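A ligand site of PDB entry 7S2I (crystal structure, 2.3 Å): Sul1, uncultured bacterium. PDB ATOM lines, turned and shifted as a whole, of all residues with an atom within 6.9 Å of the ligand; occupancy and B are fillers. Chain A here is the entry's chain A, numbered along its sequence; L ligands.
OD1 of Asp 173 is in hydrogen-bond range of N of Gly 175, 2.9 Å away. The backbone carbonyl oxygen of Val 207 sits at hydrogen-bond distance from the backbone NH of Arg 246, 3.0 Å away. The backbone carbonyl oxygen (O) of Ser 208 lies within hydrogen-bond range of the side-chain amino group (NZ) of Lys 212 (3.1 Å). The side-chain hydroxyl (OG) of Ser 208 lies within hydrogen-bond range of the guanidinium group (NH1) of Arg 246 (2.7 Å). The side-chain carboxylate (OD2) of Asp 82 lies within salt-bridge range of the guanidinium group (NH2) of Arg 246, 3.4 Å away. The backbone NH (N) of Asp 173 lies within hydrogen-bond range of the backbone carbonyl oxygen (O) of Val 124. N of Met 125 lies within hydrogen-bond range of O of Asp 102. OD2 of Asp 43 lies within salt-bridge range of NE of Arg 246, at 2.6 Å.
N1 of the ligand lies close to OD2 of Asp 82, 3.2 Å away. Ile 103 touches the ligand. Val 123 touches the ligand. Phe 179 touches the ligand (CE2 to N5, 3.4 Å). Ser 208 touches the ligand (CB to O1, 3.5 Å). The nearest printed residue that does not touch the ligand is Ser 49 (4.2 Å).
A nitrogen (N3) of the ligand is in hydrogen-bond range of the side-chain amide oxygen (OD1) of Asn 101, 2.8 Å away. NZ of Lys 212 sits at hydrogen-bond distance from O1 of the ligand (2.8 Å). OD2 of Asp 173 is in hydrogen-bond range of N4 of the ligand (2.8 Å). N1 of the ligand sits at hydrogen-bond distance from NH2 of Arg 246 (3.3 Å). SD of Met 125 lies within hydrogen-bond range of N4 of the ligand (3.3 Å).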
ATOM      1  N   ILE A   7     -19.698  -2.954   0.163  1.00  0.00           N
ATOM      2  CA  ILE A   7     -20.639  -3.564  -0.769  1.00  0.00           C
ATOM      3  C   ILE A   7     -22.035  -3.047  -0.492  1.00  0.00           C
ATOM      4  O   ILE A   7     -22.533  -3.134   0.638  1.00  0.00           O
ATOM      5  CB  ILE A   7     -20.607  -5.098  -0.658  1.00  0.00           C
ATOM      6  CG1 ILE A   7     -19.238  -5.653  -1.054  1.00  0.00           C
ATOM      7  CG2 ILE A   7     -21.705  -5.723  -1.539  1.00  0.00           C
ATOM      8  CD1 ILE A   7     -19.059  -7.129  -0.701  1.00  0.00           C
ATOM      9  N   ASP A  43     -19.683   0.414  -3.398  1.00  0.00           N
ATOM     10  CA  ASP A  43     -19.746  -0.421  -4.597  1.00  0.00           C
ATOM     11  C   ASP A  43     -21.189  -0.822  -4.849  1.00  0.00           C
ATOM     12  O   ASP A  43     -21.698  -1.768  -4.235  1.00  0.00           O
ATOM     13  CB  ASP A  43     -18.845  -1.646  -4.462  1.00  0.00           C
ATOM     14  CG  ASP A  43     -18.731  -2.449  -5.755  1.00  0.00           C
ATOM     15  OD1 ASP A  43     -18.693  -1.854  -6.851  1.00  0.00           O
ATOM     16  OD2 ASP A  43     -18.664  -3.697  -5.665  1.00  0.00           O
ATOM     17  N   SER A  49     -27.785 -11.707  -7.526  1.00  0.00           N
ATOM     18  CA  SER A  49     -27.128 -13.007  -7.493  1.00  0.00           C
ATOM     19  C   SER A  49     -27.974 -14.067  -6.796  1.00  0.00           C
ATOM     20  O   SER A  49     -27.454 -15.093  -6.346  1.00  0.00           O
ATOM     21  CB  SER A  49     -25.749 -12.887  -6.831  1.00  0.00           C
ATOM     22  OG  SER A  49     -24.802 -13.758  -7.439  1.00  0.00           O
ATOM     23  N   ASP A  82     -20.972  -1.821  -9.821  1.00  0.00           N
ATOM     24  CA  ASP A  82     -20.731  -3.261  -9.946  1.00  0.00           C
ATOM     25  C   ASP A  82     -21.713  -3.800 -11.001  1.00  0.00           C
ATOM     26  O   ASP A  82     -22.858  -4.144 -10.690  1.00  0.00           O
ATOM     27  CB  ASP A  82     -20.894  -3.924  -8.580  1.00  0.00           C
ATOM     28  CG  ASP A  82     -20.769  -5.436  -8.615  1.00  0.00           C
ATOM     29  OD1 ASP A  82     -20.425  -6.011  -9.673  1.00  0.00           O
ATOM     30  OD2 ASP A  82     -20.991  -6.062  -7.557  1.00  0.00           O
ATOM     31  N   ASN A 101     -16.610  -1.615 -11.871  1.00  0.00           N
ATOM     32  CA  ASN A 101     -16.259  -2.923 -11.331  1.00  0.00           C
ATOM     33  C   ASN A 101     -16.942  -3.986 -12.184  1.00  0.00           C
ATOM     34  O   ASN A 101     -18.170  -4.130 -12.125  1.00  0.00           O
ATOM     35  CB  ASN A 101     -16.678  -3.016  -9.857  1.00  0.00           C
ATOM     36  CG  ASN A 101     -16.307  -4.333  -9.211  1.00  0.00           C
ATOM     37  OD1 ASN A 101     -15.442  -5.053  -9.708  1.00  0.00           O
ATOM     38  ND2 ASN A 101     -16.984  -4.676  -8.107  1.00  0.00           N
ATOM     39  N   ASP A 102     -16.168  -4.710 -12.981  1.00  0.00           N
ATOM     40  CA  ASP A 102     -16.721  -5.686 -13.922  1.00  0.00           C
ATOM     41  C   ASP A 102     -16.194  -7.077 -13.604  1.00  0.00           C
ATOM     42  O   ASP A 102     -15.000  -7.348 -13.766  1.00  0.00           O
ATOM     43  CB  ASP A 102     -16.389  -5.301 -15.364  1.00  0.00           C
ATOM     44  CG  ASP A 102     -17.070  -6.217 -16.376  1.00  0.00           C
ATOM     45  OD1 ASP A 102     -17.832  -7.120 -15.949  1.00  0.00           O
ATOM     46  OD2 ASP A 102     -16.852  -6.023 -17.598  1.00  0.00           O
ATOM     47  N   ILE A 103     -17.104  -7.987 -13.227  1.00  0.00           N
ATOM     48  CA  ILE A 103     -16.708  -9.373 -12.964  1.00  0.00           C
ATOM     49  C   ILE A 103     -16.327 -10.110 -14.234  1.00  0.00           C
ATOM     50  O   ILE A 103     -15.766 -11.219 -14.167  1.00  0.00           O
ATOM     51  CB  ILE A 103     -17.838 -10.151 -12.251  1.00  0.00           C
ATOM     52  CG1 ILE A 103     -19.145 -10.057 -13.033  1.00  0.00           C
ATOM     53  CG2 ILE A 103     -18.060  -9.582 -10.840  1.00  0.00           C
ATOM     54  CD1 ILE A 103     -20.202 -11.075 -12.594  1.00  0.00           C
ATOM     55  N   VAL A 123     -11.833  -1.831 -12.162  1.00  0.00           N
ATOM     56  CA  VAL A 123     -11.565  -3.077 -11.461  1.00  0.00           C
ATOM     57  C   VAL A 123     -11.749  -4.201 -12.473  1.00  0.00           C
ATOM     58  O   VAL A 123     -12.875  -4.576 -12.816  1.00  0.00           O
ATOM     59  CB  VAL A 123     -12.493  -3.262 -10.253  1.00  0.00           C
ATOM     60  CG1 VAL A 123     -12.181  -4.587  -9.564  1.00  0.00           C
ATOM     61  CG2 VAL A 123     -12.349  -2.093  -9.297  1.00  0.00           C
ATOM     62  N   VAL A 124     -10.637  -4.738 -12.957  1.00  0.00           N
ATOM     63  CA  VAL A 124     -10.645  -5.777 -13.975  1.00  0.00           C
ATOM     64  C   VAL A 124     -10.548  -7.128 -13.260  1.00  0.00           C
ATOM     65  O   VAL A 124      -9.476  -7.501 -12.793  1.00  0.00           O
ATOM     66  CB  VAL A 124      -9.497  -5.582 -14.970  1.00  0.00           C
ATOM     67  CG1 VAL A 124      -9.596  -6.584 -16.115  1.00  0.00           C
ATOM     68  CG2 VAL A 124      -9.519  -4.150 -15.510  1.00  0.00           C
ATOM     69  N   MET A 125     -11.665  -7.842 -13.173  1.00  0.00           N
ATOM     70  CA  MET A 125     -11.678  -9.107 -12.458  1.00  0.00           C
ATOM     71  C   MET A 125     -11.439 -10.288 -13.390  1.00  0.00           C
ATOM     72  O   MET A 125     -11.995 -10.376 -14.491  1.00  0.00           O
ATOM     73  CB  MET A 125     -12.999  -9.305 -11.723  1.00  0.00           C
ATOM     74  CG  MET A 125     -12.978 -10.564 -10.899  1.00  0.00           C
ATOM     75  SD  MET A 125     -14.405 -10.706  -9.840  1.00  0.00           S
ATOM     76  CE  MET A 125     -15.092 -12.213 -10.461  1.00  0.00           C
ATOM     77  N   ASP A 173      -8.301  -7.761 -10.024  1.00  0.00           N
ATOM     78  CA  ASP A 173      -8.942  -8.657  -9.063  1.00  0.00           C
ATOM     79  C   ASP A 173      -8.749 -10.094  -9.514  1.00  0.00           C
ATOM     80  O   ASP A 173      -9.283 -10.484 -10.561  1.00  0.00           O
ATOM     81  CB  ASP A 173     -10.448  -8.326  -8.949  1.00  0.00           C
ATOM     82  CG  ASP A 173     -11.172  -9.151  -7.878  1.00  0.00           C
ATOM     83  OD1 ASP A 173     -10.644 -10.195  -7.441  1.00  0.00           O
ATOM     84  OD2 ASP A 173     -12.300  -8.759  -7.498  1.00  0.00           O
ATOM     85  N   GLY A 175     -10.138 -12.750  -8.631  1.00  0.00           N
ATOM     86  CA  GLY A 175     -11.290 -13.618  -8.493  1.00  0.00           C
ATOM     87  C   GLY A 175     -11.142 -14.498  -7.278  1.00  0.00           C
ATOM     88  O   GLY A 175     -10.021 -14.908  -6.937  1.00  0.00           O
ATOM     89  N   MET A 176     -12.240 -14.796  -6.597  1.00  0.00           N
ATOM     90  CA  MET A 176     -12.217 -15.677  -5.433  1.00  0.00           C
ATOM     91  C   MET A 176     -13.484 -16.531  -5.404  1.00  0.00           C
ATOM     92  O   MET A 176     -14.484 -16.220  -6.059  1.00  0.00           O
ATOM     93  CB  MET A 176     -12.062 -14.904  -4.123  1.00  0.00           C
ATOM     94  CG  MET A 176     -10.713 -14.254  -4.027  1.00  0.00           C
ATOM     95  SD  MET A 176      -9.539 -15.437  -3.338  1.00  0.00           S
ATOM     96  CE  MET A 176      -7.997 -14.601  -3.709  1.00  0.00           C
ATOM     97  N   GLY A 177     -13.428 -17.597  -4.619  1.00  0.00           N
ATOM     98  CA  GLY A 177     -14.560 -18.505  -4.518  1.00  0.00           C
ATOM     99  C   GLY A 177     -14.861 -19.185  -5.836  1.00  0.00           C
ATOM    100  O   GLY A 177     -13.964 -19.623  -6.563  1.00  0.00           O
ATOM    101  N   PHE A 179     -15.799 -17.951  -8.542  1.00  0.00           N
ATOM    102  CA  PHE A 179     -15.262 -17.317  -9.733  1.00  0.00           C
ATOM    103  C   PHE A 179     -13.922 -17.912 -10.142  1.00  0.00           C
ATOM    104  O   PHE A 179     -13.540 -17.808 -11.313  1.00  0.00           O
ATOM    105  CB  PHE A 179     -15.115 -15.808  -9.525  1.00  0.00           C
ATOM    106  CG  PHE A 179     -16.427 -15.099  -9.390  1.00  0.00           C
ATOM    107  CD1 PHE A 179     -17.327 -15.060 -10.436  1.00  0.00           C
ATOM    108  CD2 PHE A 179     -16.764 -14.486  -8.189  1.00  0.00           C
ATOM    109  CE1 PHE A 179     -18.537 -14.387 -10.308  1.00  0.00           C
ATOM    110  CE2 PHE A 179     -17.973 -13.816  -8.048  1.00  0.00           C
ATOM    111  CZ  PHE A 179     -18.857 -13.775  -9.110  1.00  0.00           C
ATOM    112  N   LEU A 206      -6.956  -5.756  -6.066  1.00  0.00           N
ATOM    113  CA  LEU A 206      -8.147  -5.760  -5.241  1.00  0.00           C
ATOM    114  C   LEU A 206      -8.548  -7.210  -4.980  1.00  0.00           C
ATOM    115  O   LEU A 206      -8.395  -8.064  -5.856  1.00  0.00           O
ATOM    116  CB  LEU A 206      -9.310  -5.013  -5.911  1.00  0.00           C
ATOM    117  CG  LEU A 206     -10.652  -4.904  -5.185  1.00  0.00           C
ATOM    118  CD1 LEU A 206     -11.385  -3.606  -5.534  1.00  0.00           C
ATOM    119  CD2 LEU A 206     -11.544  -6.094  -5.516  1.00  0.00           C
ATOM    120  N   VAL A 207      -9.040  -7.491  -3.779  1.00  0.00           N
ATOM    121  CA  VAL A 207      -9.645  -8.789  -3.480  1.00  0.00           C
ATOM    122  C   VAL A 207     -11.017  -8.582  -2.856  1.00  0.00           C
ATOM    123  O   VAL A 207     -11.297  -7.557  -2.235  1.00  0.00           O
ATOM    124  CB  VAL A 207      -8.771  -9.671  -2.546  1.00  0.00           C
ATOM    125  CG1 VAL A 207      -7.481 -10.078  -3.245  1.00  0.00           C
ATOM    126  CG2 VAL A 207      -8.506  -8.953  -1.257  1.00  0.00           C
ATOM    127  N   SER A 208     -11.864  -9.580  -3.036  1.00  0.00           N
ATOM    128  CA  SER A 208     -13.194  -9.599  -2.428  1.00  0.00           C
ATOM    129  C   SER A 208     -13.405 -11.030  -1.926  1.00  0.00           C
ATOM    130  O   SER A 208     -13.883 -11.890  -2.667  1.00  0.00           O
ATOM    131  CB  SER A 208     -14.277  -9.173  -3.403  1.00  0.00           C
ATOM    132  OG  SER A 208     -15.510  -8.977  -2.740  1.00  0.00           O
ATOM    133  N   VAL A 209     -13.024 -11.271  -0.665  1.00  0.00           N
ATOM    134  CA  VAL A 209     -13.203 -12.586  -0.054  1.00  0.00           C
ATOM    135  C   VAL A 209     -14.445 -12.648   0.820  1.00  0.00           C
ATOM    136  O   VAL A 209     -14.899 -13.761   1.151  1.00  0.00           O
ATOM    137  CB  VAL A 209     -11.983 -12.980   0.796  1.00  0.00           C
ATOM    138  CG1 VAL A 209     -10.758 -13.121  -0.073  1.00  0.00           C
ATOM    139  CG2 VAL A 209     -11.776 -11.931   1.888  1.00  0.00           C
ATOM    140  N   LYS A 212     -17.372 -15.434   0.998  1.00  0.00           N
ATOM    141  CA  LYS A 212     -17.303 -16.333  -0.138  1.00  0.00           C
ATOM    142  C   LYS A 212     -17.369 -17.803   0.298  1.00  0.00           C
ATOM    143  O   LYS A 212     -16.930 -18.179   1.396  1.00  0.00           O
ATOM    144  CB  LYS A 212     -16.022 -16.085  -0.943  1.00  0.00           C
ATOM    145  CG  LYS A 212     -15.974 -14.751  -1.695  1.00  0.00           C
ATOM    146  CD  LYS A 212     -16.588 -14.837  -3.070  1.00  0.00           C
ATOM    147  CE  LYS A 212     -15.984 -13.815  -4.006  1.00  0.00           C
ATOM    148  NZ  LYS A 212     -16.655 -12.491  -3.868  1.00  0.00           N
ATOM    149  N   ARG A 246     -12.837  -5.248  -1.193  1.00  0.00           N
ATOM    150  CA  ARG A 246     -14.295  -5.167  -1.317  1.00  0.00           C
ATOM    151  C   ARG A 246     -14.905  -6.045  -0.230  1.00  0.00           C
ATOM    152  O   ARG A 246     -14.636  -7.250  -0.190  1.00  0.00           O
ATOM    153  CB  ARG A 246     -14.701  -5.643  -2.714  1.00  0.00           C
ATOM    154  CG  ARG A 246     -16.172  -5.478  -3.021  1.00  0.00           C
ATOM    155  CD  ARG A 246     -16.452  -5.700  -4.510  1.00  0.00           C
ATOM    156  NE  ARG A 246     -17.855  -6.012  -4.780  1.00  0.00           N
ATOM    157  CZ  ARG A 246     -18.510  -7.092  -4.363  1.00  0.00           C
ATOM    158  NH1 ARG A 246     -17.884  -8.121  -3.823  1.00  0.00           N
ATOM    159  NH2 ARG A 246     -19.834  -7.139  -4.532  1.00  0.00           N
ATOM    160  N   HIS A 248     -18.300  -6.756   2.841  1.00  0.00           N
ATOM    161  CA  HIS A 248     -19.600  -6.518   3.458  1.00  0.00           C
ATOM    162  C   HIS A 248     -19.497  -5.754   4.779  1.00  0.00           C
ATOM    163  O   HIS A 248     -20.475  -5.136   5.203  1.00  0.00           O
ATOM    164  CB  HIS A 248     -20.326  -7.846   3.704  1.00  0.00           C
ATOM    165  CG  HIS A 248     -20.653  -8.595   2.450  1.00  0.00           C
ATOM    166  ND1 HIS A 248     -19.822  -9.565   1.917  1.00  0.00           N
ATOM    167  CD2 HIS A 248     -21.707  -8.503   1.600  1.00  0.00           C
ATOM    168  CE1 HIS A 248     -20.349 -10.032   0.804  1.00  0.00           C
ATOM    169  NE2 HIS A 248     -21.495  -9.402   0.594  1.00  0.00           N
HETATM  170  C1  LIG L   1     -19.998  -9.632  -6.856  1.00  0.00           C
HETATM  171  N1  LIG L   1     -19.114  -8.640  -7.340  1.00  0.00           N
HETATM  172  C2  LIG L   1     -17.778  -8.827  -7.223  1.00  0.00           C
HETATM  173  N2  LIG L   1     -16.928  -7.895  -7.660  1.00  0.00           N
HETATM  174  C3  LIG L   1     -15.583  -8.056  -7.581  1.00  0.00           C
HETATM  175  N3  LIG L   1     -14.712  -7.141  -8.026  1.00  0.00           N
HETATM  176  C4  LIG L   1     -17.297  -9.990  -6.636  1.00  0.00           C
HETATM  177  C5  LIG L   1     -15.916 -10.189  -6.528  1.00  0.00           C
HETATM  178  N4  LIG L   1     -15.057  -9.217  -7.006  1.00  0.00           N
HETATM  179  O1  LIG L   1     -15.422 -11.199  -6.025  1.00  0.00           O
HETATM  180  N5  LIG L   1     -18.146 -10.927  -6.185  1.00  0.00           N
HETATM  181  C6  LIG L   1     -19.485 -10.785  -6.255  1.00  0.00           C
HETATM  182  C7  LIG L   1     -20.350 -11.782  -5.760  1.00  0.00           C
HETATM  183  O2  LIG L   1     -21.652 -11.477  -5.953  1.00  0.00           O
